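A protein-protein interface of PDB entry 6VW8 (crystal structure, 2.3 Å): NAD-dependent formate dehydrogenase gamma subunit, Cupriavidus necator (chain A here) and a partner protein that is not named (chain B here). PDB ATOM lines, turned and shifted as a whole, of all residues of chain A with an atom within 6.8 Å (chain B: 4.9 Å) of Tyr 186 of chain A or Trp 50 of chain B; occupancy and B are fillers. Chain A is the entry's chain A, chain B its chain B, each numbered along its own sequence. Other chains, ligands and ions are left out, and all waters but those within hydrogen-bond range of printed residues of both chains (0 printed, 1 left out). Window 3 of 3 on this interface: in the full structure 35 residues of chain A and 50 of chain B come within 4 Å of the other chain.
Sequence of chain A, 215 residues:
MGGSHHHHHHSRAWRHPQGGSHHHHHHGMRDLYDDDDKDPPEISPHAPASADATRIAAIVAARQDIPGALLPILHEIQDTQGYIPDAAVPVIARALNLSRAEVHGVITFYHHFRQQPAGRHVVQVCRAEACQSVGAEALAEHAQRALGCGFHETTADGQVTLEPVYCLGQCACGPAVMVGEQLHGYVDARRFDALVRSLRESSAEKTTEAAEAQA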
ATOM      1  N   VAL A 134     -23.673  11.743 -18.283  1.00  0.00           N
ATOM      2  CA  VAL A 134     -24.151  10.375 -18.156  1.00  0.00           C
ATOM      3  C   VAL A 134     -23.496   9.739 -16.943  1.00  0.00           C
ATOM      4  O   VAL A 134     -23.360   8.512 -16.874  1.00  0.00           O
ATOM      5  CB  VAL A 134     -23.910   9.555 -19.433  1.00  0.00           C
ATOM      6  CG1 VAL A 134     -24.875  10.007 -20.528  1.00  0.00           C
ATOM      7  CG2 VAL A 134     -22.431   9.650 -19.888  1.00  0.00           C
ATOM      8  N   GLN A 170     -14.661  10.174 -26.531  1.00  0.00           N
ATOM      9  CA  GLN A 170     -15.647   9.100 -26.441  1.00  0.00           C
ATOM     10  C   GLN A 170     -16.969   9.640 -25.902  1.00  0.00           C
ATOM     11  O   GLN A 170     -17.699   8.947 -25.179  1.00  0.00           O
ATOM     12  CB  GLN A 170     -15.127   7.963 -25.561  1.00  0.00           C
ATOM     13  CG  GLN A 170     -13.675   7.548 -25.847  1.00  0.00           C
ATOM     14  CD  GLN A 170     -13.483   7.037 -27.260  1.00  0.00           C
ATOM     15  OE1 GLN A 170     -14.332   6.306 -27.776  1.00  0.00           O
ATOM     16  NE2 GLN A 170     -12.375   7.432 -27.903  1.00  0.00           N
ATOM     17  N   ALA A 172     -19.912  10.415 -26.899  1.00  0.00           N
ATOM     18  CA  ALA A 172     -21.184   9.762 -27.199  1.00  0.00           C
ATOM     19  C   ALA A 172     -21.315   8.378 -26.568  1.00  0.00           C
ATOM     20  O   ALA A 172     -22.347   7.723 -26.749  1.00  0.00           O
ATOM     21  CB  ALA A 172     -21.384   9.658 -28.718  1.00  0.00           C
ATOM     22  N   CYS A 173     -20.300   7.889 -25.874  1.00  0.00           N
ATOM     23  CA  CYS A 173     -20.382   6.540 -25.348  1.00  0.00           C
ATOM     24  C   CYS A 173     -19.867   6.518 -23.909  1.00  0.00           C
ATOM     25  O   CYS A 173     -19.230   5.543 -23.473  1.00  0.00           O
ATOM     26  CB  CYS A 173     -19.703   5.527 -26.317  1.00  0.00           C
ATOM     27  SG  CYS A 173     -17.949   5.208 -26.190  1.00  0.00           S
ATOM     28  N   GLY A 174     -20.092   7.613 -23.175  1.00  0.00           N
ATOM     29  CA  GLY A 174     -19.568   7.740 -21.837  1.00  0.00           C
ATOM     30  C   GLY A 174     -20.449   7.042 -20.826  1.00  0.00           C
ATOM     31  O   GLY A 174     -21.498   6.494 -21.153  1.00  0.00           O
ATOM     32  N   PRO A 175     -20.012   7.042 -19.555  1.00  0.00           N
ATOM     33  CA  PRO A 175     -18.741   7.579 -19.050  1.00  0.00           C
ATOM     34  C   PRO A 175     -17.539   6.808 -19.584  1.00  0.00           C
ATOM     35  O   PRO A 175     -17.568   5.570 -19.626  1.00  0.00           O
ATOM     36  CB  PRO A 175     -18.860   7.403 -17.521  1.00  0.00           C
ATOM     37  CG  PRO A 175     -20.290   7.145 -17.250  1.00  0.00           C
ATOM     38  CD  PRO A 175     -20.840   6.486 -18.472  1.00  0.00           C
ATOM     39  N   ALA A 176     -16.490   7.515 -19.986  1.00  0.00           N
ATOM     40  CA  ALA A 176     -15.355   6.865 -20.621  1.00  0.00           C
ATOM     41  C   ALA A 176     -14.202   6.678 -19.644  1.00  0.00           C
ATOM     42  O   ALA A 176     -13.981   7.493 -18.742  1.00  0.00           O
ATOM     43  CB  ALA A 176     -14.886   7.673 -21.838  1.00  0.00           C
ATOM     44  N   VAL A 177     -13.460   5.592 -19.846  1.00  0.00           N
ATOM     45  CA  VAL A 177     -12.272   5.257 -19.062  1.00  0.00           C
ATOM     46  C   VAL A 177     -11.187   4.753 -20.004  1.00  0.00           C
ATOM     47  O   VAL A 177     -11.472   3.983 -20.928  1.00  0.00           O
ATOM     48  CB  VAL A 177     -12.595   4.197 -17.990  1.00  0.00           C
ATOM     49  CG1 VAL A 177     -11.338   3.675 -17.371  1.00  0.00           C
ATOM     50  CG2 VAL A 177     -13.552   4.788 -16.931  1.00  0.00           C
ATOM     51  N   HIS A 184     -12.663   2.147 -22.508  1.00  0.00           N
ATOM     52  CA  HIS A 184     -13.889   1.548 -22.005  1.00  0.00           C
ATOM     53  C   HIS A 184     -14.987   2.600 -22.029  1.00  0.00           C
ATOM     54  O   HIS A 184     -14.782   3.724 -21.559  1.00  0.00           O
ATOM     55  CB  HIS A 184     -13.676   0.996 -20.589  1.00  0.00           C
ATOM     56  CG  HIS A 184     -12.635  -0.078 -20.522  1.00  0.00           C
ATOM     57  ND1 HIS A 184     -12.916  -1.400 -20.793  1.00  0.00           N
ATOM     58  CD2 HIS A 184     -11.311  -0.022 -20.246  1.00  0.00           C
ATOM     59  CE1 HIS A 184     -11.809  -2.114 -20.679  1.00  0.00           C
ATOM     60  NE2 HIS A 184     -10.823  -1.302 -20.344  1.00  0.00           N
ATOM     61  N   GLY A 185     -16.147   2.239 -22.584  1.00  0.00           N
ATOM     62  CA  GLY A 185     -17.287   3.125 -22.661  1.00  0.00           C
ATOM     63  C   GLY A 185     -18.426   2.647 -21.774  1.00  0.00           C
ATOM     64  O   GLY A 185     -18.395   1.544 -21.222  1.00  0.00           O
ATOM     65  N   TYR A 186     -19.444   3.513 -21.644  1.00  0.00           N
ATOM     66  CA  TYR A 186     -20.641   3.235 -20.838  1.00  0.00           C
ATOM     67  C   TYR A 186     -20.275   2.659 -19.477  1.00  0.00           C
ATOM     68  O   TYR A 186     -20.867   1.676 -19.024  1.00  0.00           O
ATOM     69  CB  TYR A 186     -21.598   2.259 -21.539  1.00  0.00           C
ATOM     70  CG  TYR A 186     -22.044   2.578 -22.948  1.00  0.00           C
ATOM     71  CD1 TYR A 186     -22.680   3.780 -23.252  1.00  0.00           C
ATOM     72  CD2 TYR A 186     -21.885   1.649 -23.963  1.00  0.00           C
ATOM     73  CE1 TYR A 186     -23.108   4.059 -24.551  1.00  0.00           C
ATOM     74  CE2 TYR A 186     -22.305   1.921 -25.255  1.00  0.00           C
ATOM     75  CZ  TYR A 186     -22.911   3.132 -25.541  1.00  0.00           C
ATOM     76  OH  TYR A 186     -23.344   3.408 -26.818  1.00  0.00           O
ATOM     77  N   VAL A 187     -19.275   3.230 -18.823  1.00  0.00           N
ATOM     78  CA  VAL A 187     -18.718   2.608 -17.626  1.00  0.00           C
ATOM     79  C   VAL A 187     -19.529   3.036 -16.412  1.00  0.00           C
ATOM     80  O   VAL A 187     -19.657   4.230 -16.125  1.00  0.00           O
ATOM     81  CB  VAL A 187     -17.236   2.949 -17.438  1.00  0.00           C
ATOM     82  CG1 VAL A 187     -16.708   2.246 -16.180  1.00  0.00           C
ATOM     83  CG2 VAL A 187     -16.436   2.524 -18.665  1.00  0.00           C
ATOM     84  N   ASP A 188     -20.088   2.059 -15.710  1.00  0.00           N
ATOM     85  CA  ASP A 188     -20.717   2.277 -14.426  1.00  0.00           C
ATOM     86  C   ASP A 188     -19.878   1.597 -13.348  1.00  0.00           C
ATOM     87  O   ASP A 188     -18.749   1.151 -13.595  1.00  0.00           O
ATOM     88  CB  ASP A 188     -22.161   1.769 -14.449  1.00  0.00           C
ATOM     89  CG  ASP A 188     -22.267   0.269 -14.722  1.00  0.00           C
ATOM     90  OD1 ASP A 188     -21.226  -0.424 -14.845  1.00  0.00           O
ATOM     91  OD2 ASP A 188     -23.415  -0.217 -14.812  1.00  0.00           O
ATOM     92  N   ARG A 191     -19.158  -2.238 -14.116  1.00  0.00           N
ATOM     93  CA  ARG A 191     -18.185  -2.439 -15.187  1.00  0.00           C
ATOM     94  C   ARG A 191     -16.804  -1.953 -14.764  1.00  0.00           C
ATOM     95  O   ARG A 191     -15.792  -2.556 -15.139  1.00  0.00           O
ATOM     96  CB  ARG A 191     -18.646  -1.736 -16.467  1.00  0.00           C
ATOM     97  CG  ARG A 191     -19.865  -2.388 -17.126  1.00  0.00           C
ATOM     98  CD  ARG A 191     -20.373  -1.594 -18.334  1.00  0.00           C
ATOM     99  NE  ARG A 191     -19.470  -1.681 -19.488  1.00  0.00           N
ATOM    100  CZ  ARG A 191     -19.658  -2.487 -20.534  1.00  0.00           C
ATOM    101  NH1 ARG A 191     -20.719  -3.286 -20.578  1.00  0.00           N
ATOM    102  NH2 ARG A 191     -18.786  -2.496 -21.536  1.00  0.00           N
ATOM    103  N   LEU B  18     -15.986  -0.356 -27.330  1.00  0.00           N
ATOM    104  CA  LEU B  18     -17.187  -1.159 -27.164  1.00  0.00           C
ATOM    105  C   LEU B  18     -17.017  -2.590 -27.684  1.00  0.00           C
ATOM    106  O   LEU B  18     -18.015  -3.286 -27.901  1.00  0.00           O
ATOM    107  CB  LEU B  18     -18.373  -0.469 -27.838  1.00  0.00           C
ATOM    108  CG  LEU B  18     -18.642   0.996 -27.449  1.00  0.00           C
ATOM    109  CD1 LEU B  18     -19.689   1.664 -28.359  1.00  0.00           C
ATOM    110  CD2 LEU B  18     -19.046   1.111 -25.989  1.00  0.00           C
ATOM    111  N   MET B  48     -22.292   6.177 -35.952  1.00  0.00           N
ATOM    112  CA  MET B  48     -23.571   5.942 -35.284  1.00  0.00           C
ATOM    113  C   MET B  48     -23.274   5.105 -34.043  1.00  0.00           C
ATOM    114  O   MET B  48     -23.471   3.891 -34.018  1.00  0.00           O
ATOM    115  CB  MET B  48     -24.576   5.241 -36.231  1.00  0.00           C
ATOM    116  CG  MET B  48     -25.001   6.062 -37.452  1.00  0.00           C
ATOM    117  SD  MET B  48     -26.142   5.163 -38.548  1.00  0.00           S
ATOM    118  CE  MET B  48     -24.996   4.119 -39.442  1.00  0.00           C
ATOM    119  N   PHE B  49     -22.799   5.774 -32.996  1.00  0.00           N
ATOM    120  CA  PHE B  49     -22.116   5.075 -31.912  1.00  0.00           C
ATOM    121  C   PHE B  49     -23.035   4.205 -31.071  1.00  0.00           C
ATOM    122  O   PHE B  49     -22.557   3.246 -30.474  1.00  0.00           O
ATOM    123  CB  PHE B  49     -21.360   6.087 -31.057  1.00  0.00           C
ATOM    124  CG  PHE B  49     -20.211   6.727 -31.784  1.00  0.00           C
ATOM    125  CD1 PHE B  49     -19.538   6.029 -32.775  1.00  0.00           C
ATOM    126  CD2 PHE B  49     -19.817   8.019 -31.498  1.00  0.00           C
ATOM    127  CE1 PHE B  49     -18.468   6.598 -33.446  1.00  0.00           C
ATOM    128  CE2 PHE B  49     -18.751   8.596 -32.170  1.00  0.00           C
ATOM    129  CZ  PHE B  49     -18.071   7.892 -33.145  1.00  0.00           C
ATOM    130  N   TRP B  50     -24.330   4.495 -31.009  1.00  0.00           N
ATOM    131  CA  TRP B  50     -25.235   3.599 -30.296  1.00  0.00           C
ATOM    132  C   TRP B  50     -25.417   2.261 -31.020  1.00  0.00           C
ATOM    133  O   TRP B  50     -25.962   1.314 -30.434  1.00  0.00           O
ATOM    134  CB  TRP B  50     -26.589   4.288 -30.068  1.00  0.00           C
ATOM    135  CG  TRP B  50     -27.433   4.280 -31.278  1.00  0.00           C
ATOM    136  CD1 TRP B  50     -28.448   3.420 -31.553  1.00  0.00           C
ATOM    137  CD2 TRP B  50     -27.321   5.147 -32.411  1.00  0.00           C
ATOM    138  NE1 TRP B  50     -28.978   3.694 -32.789  1.00  0.00           N
ATOM    139  CE2 TRP B  50     -28.305   4.751 -33.337  1.00  0.00           C
ATOM    140  CE3 TRP B  50     -26.480   6.211 -32.736  1.00  0.00           C
ATOM    141  CZ2 TRP B  50     -28.486   5.391 -34.559  1.00  0.00           C
ATOM    142  CZ3 TRP B  50     -26.653   6.845 -33.945  1.00  0.00           C
ATOM    143  CH2 TRP B  50     -27.652   6.434 -34.847  1.00  0.00           C
ATOM    144  N   LEU B  51     -24.988   2.167 -32.276  1.00  0.00           N
ATOM    145  CA  LEU B  51     -24.937   0.901 -33.001  1.00  0.00           C
ATOM    146  C   LEU B  51     -23.532   0.288 -33.045  1.00  0.00           C
ATOM    147  O   LEU B  51     -23.348  -0.773 -33.650  1.00  0.00           O
ATOM    148  CB  LEU B  51     -25.472   1.101 -34.424  1.00  0.00           C
ATOM    149  CG  LEU B  51     -26.912   1.648 -34.530  1.00  0.00           C
ATOM    150  CD1 LEU B  51     -27.372   1.688 -35.977  1.00  0.00           C
ATOM    151  CD2 LEU B  51     -27.879   0.831 -33.701  1.00  0.00           C
ATOM    152  N   GLU B  52     -22.518   0.924 -32.394  1.00  0.00           N
ATOM    153  CA  GLU B  52     -21.227   0.247 -32.485  1.00  0.00           C
ATOM    154  C   GLU B  52     -21.101  -0.814 -31.398  1.00  0.00           C
ATOM    155  O   GLU B  52     -21.643  -0.651 -30.298  1.00  0.00           O
ATOM    156  CB  GLU B  52     -20.073   1.242 -32.346  1.00  0.00           C
ATOM    157  CG  GLU B  52     -19.854   2.167 -33.550  1.00  0.00           C
ATOM    158  CD  GLU B  52     -19.417   1.435 -34.809  1.00  0.00           C
ATOM    159  OE1 GLU B  52     -19.170   0.213 -34.748  1.00  0.00           O
ATOM    160  OE2 GLU B  52     -19.288   2.095 -35.864  1.00  0.00           O
ATOM    161  N   PRO B  68     -25.996  -3.006 -32.140  1.00  0.00           N
ATOM    162  CA  PRO B  68     -24.571  -3.151 -31.795  1.00  0.00           C
ATOM    163  C   PRO B  68     -24.184  -4.628 -31.597  1.00  0.00           C
ATOM    164  O   PRO B  68     -24.946  -5.352 -30.992  1.00  0.00           O
ATOM    165  CB  PRO B  68     -24.451  -2.385 -30.480  1.00  0.00           C
ATOM    166  CG  PRO B  68     -25.811  -2.582 -29.827  1.00  0.00           C
ATOM    167  CD  PRO B  68     -26.801  -2.555 -30.983  1.00  0.00           C
ATOM    168  N   PHE B 100     -30.589   8.252 -40.171  1.00  0.00           N
ATOM    169  CA  PHE B 100     -29.589   9.062 -39.478  1.00  0.00           C
ATOM    170  C   PHE B 100     -28.370   9.308 -40.366  1.00  0.00           C
ATOM    171  O   PHE B 100     -27.804  10.414 -40.390  1.00  0.00           O
ATOM    172  CB  PHE B 100     -29.198   8.336 -38.181  1.00  0.00           C
ATOM    173  CG  PHE B 100     -28.205   9.081 -37.300  1.00  0.00           C
ATOM    174  CD1 PHE B 100     -26.852   9.160 -37.636  1.00  0.00           C
ATOM    175  CD2 PHE B 100     -28.618   9.638 -36.090  1.00  0.00           C
ATOM    176  CE1 PHE B 100     -25.945   9.817 -36.809  1.00  0.00           C
ATOM    177  CE2 PHE B 100     -27.722  10.297 -35.259  1.00  0.00           C
ATOM    178  CZ  PHE B 100     -26.383  10.375 -35.615  1.00  0.00           C
ATOM    179  N   LYS B 349     -29.668   9.640 -26.861  1.00  0.00           N
ATOM    180  CA  LYS B 349     -29.965   8.240 -27.175  1.00  0.00           C
ATOM    181  C   LYS B 349     -29.158   7.733 -28.370  1.00  0.00           C
ATOM    182  O   LYS B 349     -28.671   6.592 -28.358  1.00  0.00           O
ATOM    183  CB  LYS B 349     -31.450   8.049 -27.447  1.00  0.00           C
ATOM    184  CG  LYS B 349     -31.875   6.580 -27.409  1.00  0.00           C
ATOM    185  CD  LYS B 349     -32.856   6.246 -28.530  1.00  0.00           C
ATOM    186  CE  LYS B 349     -33.997   5.374 -28.027  1.00  0.00           C
ATOM    187  NZ  LYS B 349     -35.117   5.330 -29.015  1.00  0.00           N
ATOM    188  N   GLN B 350     -29.057   8.534 -29.429  1.00  0.00           N
ATOM    189  CA  GLN B 350     -28.397   8.158 -30.674  1.00  0.00           C
ATOM    190  C   GLN B 350     -27.332   9.200 -30.944  1.00  0.00           C
ATOM    191  O   GLN B 350     -27.526  10.100 -31.763  1.00  0.00           O
ATOM    192  CB  GLN B 350     -29.388   8.038 -31.844  1.00  0.00           C
ATOM    193  CG  GLN B 350     -30.527   7.059 -31.561  1.00  0.00           C
ATOM    194  CD  GLN B 350     -31.517   6.910 -32.705  1.00  0.00           C
ATOM    195  OE1 GLN B 350     -31.616   7.769 -33.574  1.00  0.00           O
ATOM    196  NE2 GLN B 350     -32.256   5.808 -32.704  1.00  0.00           N
ATOM    197  N   GLY B 351     -26.188   9.053 -30.262  1.00  0.00           N
ATOM    198  CA  GLY B 351     -25.082   9.969 -30.413  1.00  0.00           C
ATOM    199  C   GLY B 351     -24.143   9.580 -31.539  1.00  0.00           C
ATOM    200  O   GLY B 351     -24.162   8.455 -32.034  1.00  0.00           O
ATOM    201  N   ARG B 374     -30.566   9.817 -23.401  1.00  0.00           N
ATOM    202  CA  ARG B 374     -30.328   8.411 -23.107  1.00  0.00           C
ATOM    203  C   ARG B 374     -31.135   7.970 -21.893  1.00  0.00           C
ATOM    204  O   ARG B 374     -31.635   6.841 -21.853  1.00  0.00           O
ATOM    205  CB  ARG B 374     -28.832   8.171 -22.884  1.00  0.00           C
ATOM    206  CG  ARG B 374     -28.508   6.788 -22.359  1.00  0.00           C
ATOM    207  CD  ARG B 374     -26.996   6.573 -22.321  1.00  0.00           C
ATOM    208  NE  ARG B 374     -26.383   7.099 -23.534  1.00  0.00           N
ATOM    209  CZ  ARG B 374     -25.075   7.247 -23.721  1.00  0.00           C
ATOM    210  NH1 ARG B 374     -24.203   6.898 -22.774  1.00  0.00           N
ATOM    211  NH2 ARG B 374     -24.642   7.759 -24.865  1.00  0.00           N
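O of Ala 172 of chain A is in hydrogen-bond range of NH2 of Arg 374 of chain B (3.0 Å).
The guanidinium group (NH1) of Arg 374 of chain B lies within hydrogen-bond range of the backbone carbonyl oxygen (O) of Gly 174 of chain A (3.2 Å).
N of Tyr 186 of chain A lies within hydrogen-bond range of O of Cys 173 of chain A, 2.7 Å away.
O of Pro 175 of chain A lies within hydrogen-bond range of N of Tyr 186 of chain A.
N of Phe 49 of chain B is in hydrogen-bond range of O of Gly 351 of chain B (3.2 Å).
Tyr 186 of chain A touches just these residues of chain B: Leu 18 (3.4 Å), Phe 49 (3.7 Å), Trp 50 (3.96 Å) and Arg 374 (3.5 Å).
Trp 50 of chain B touches just one residue of chain A: Tyr 186 (3.96 Å).
Printed residues of chain A within 4 Å of Arg 374 of chain B: Val 134, Ala 172, Gly 174 and Tyr 186.
Of the printed residues of chain B, Val 134 of chain A touches Arg 374.
Printed residues of chain B within 4 Å of Gly 174 of chain A: Arg 374 (3.2 Å).
Glu 52 of chain B touches none of the printed residues of chain A.
Among the printed residues, merely in contact across the chains: Tyr 186 of chain A with Leu 18 of chain B, Tyr 186 of chain A with Arg 374 of chain B, Ala 172 of chain A with Phe 49 of chain B, Tyr 186 of chain A with Phe 49 of chain B, Val 134 of chain A with Arg 374 of chain B, Ala 172 of chain A with Gly 351 of chain B and Tyr 186 of chain A with Trp 50 of chain B.
Hydrophobic or aromatic side chains of chain B that line the printed part of chain A: Leu 18 and Phe 49.
Of the 14 printed residues of chain A, 4 touch a printed residue of chain B.
Hydrophobic or aromatic side chains of chain A that line the printed part of chain B: Val 134, Ala 172 and Tyr 186.
Among the printed residues, no Asp or Glu carboxylate lies within 4 Å of a Lys or Arg side-chain nitrogen of the other chain.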
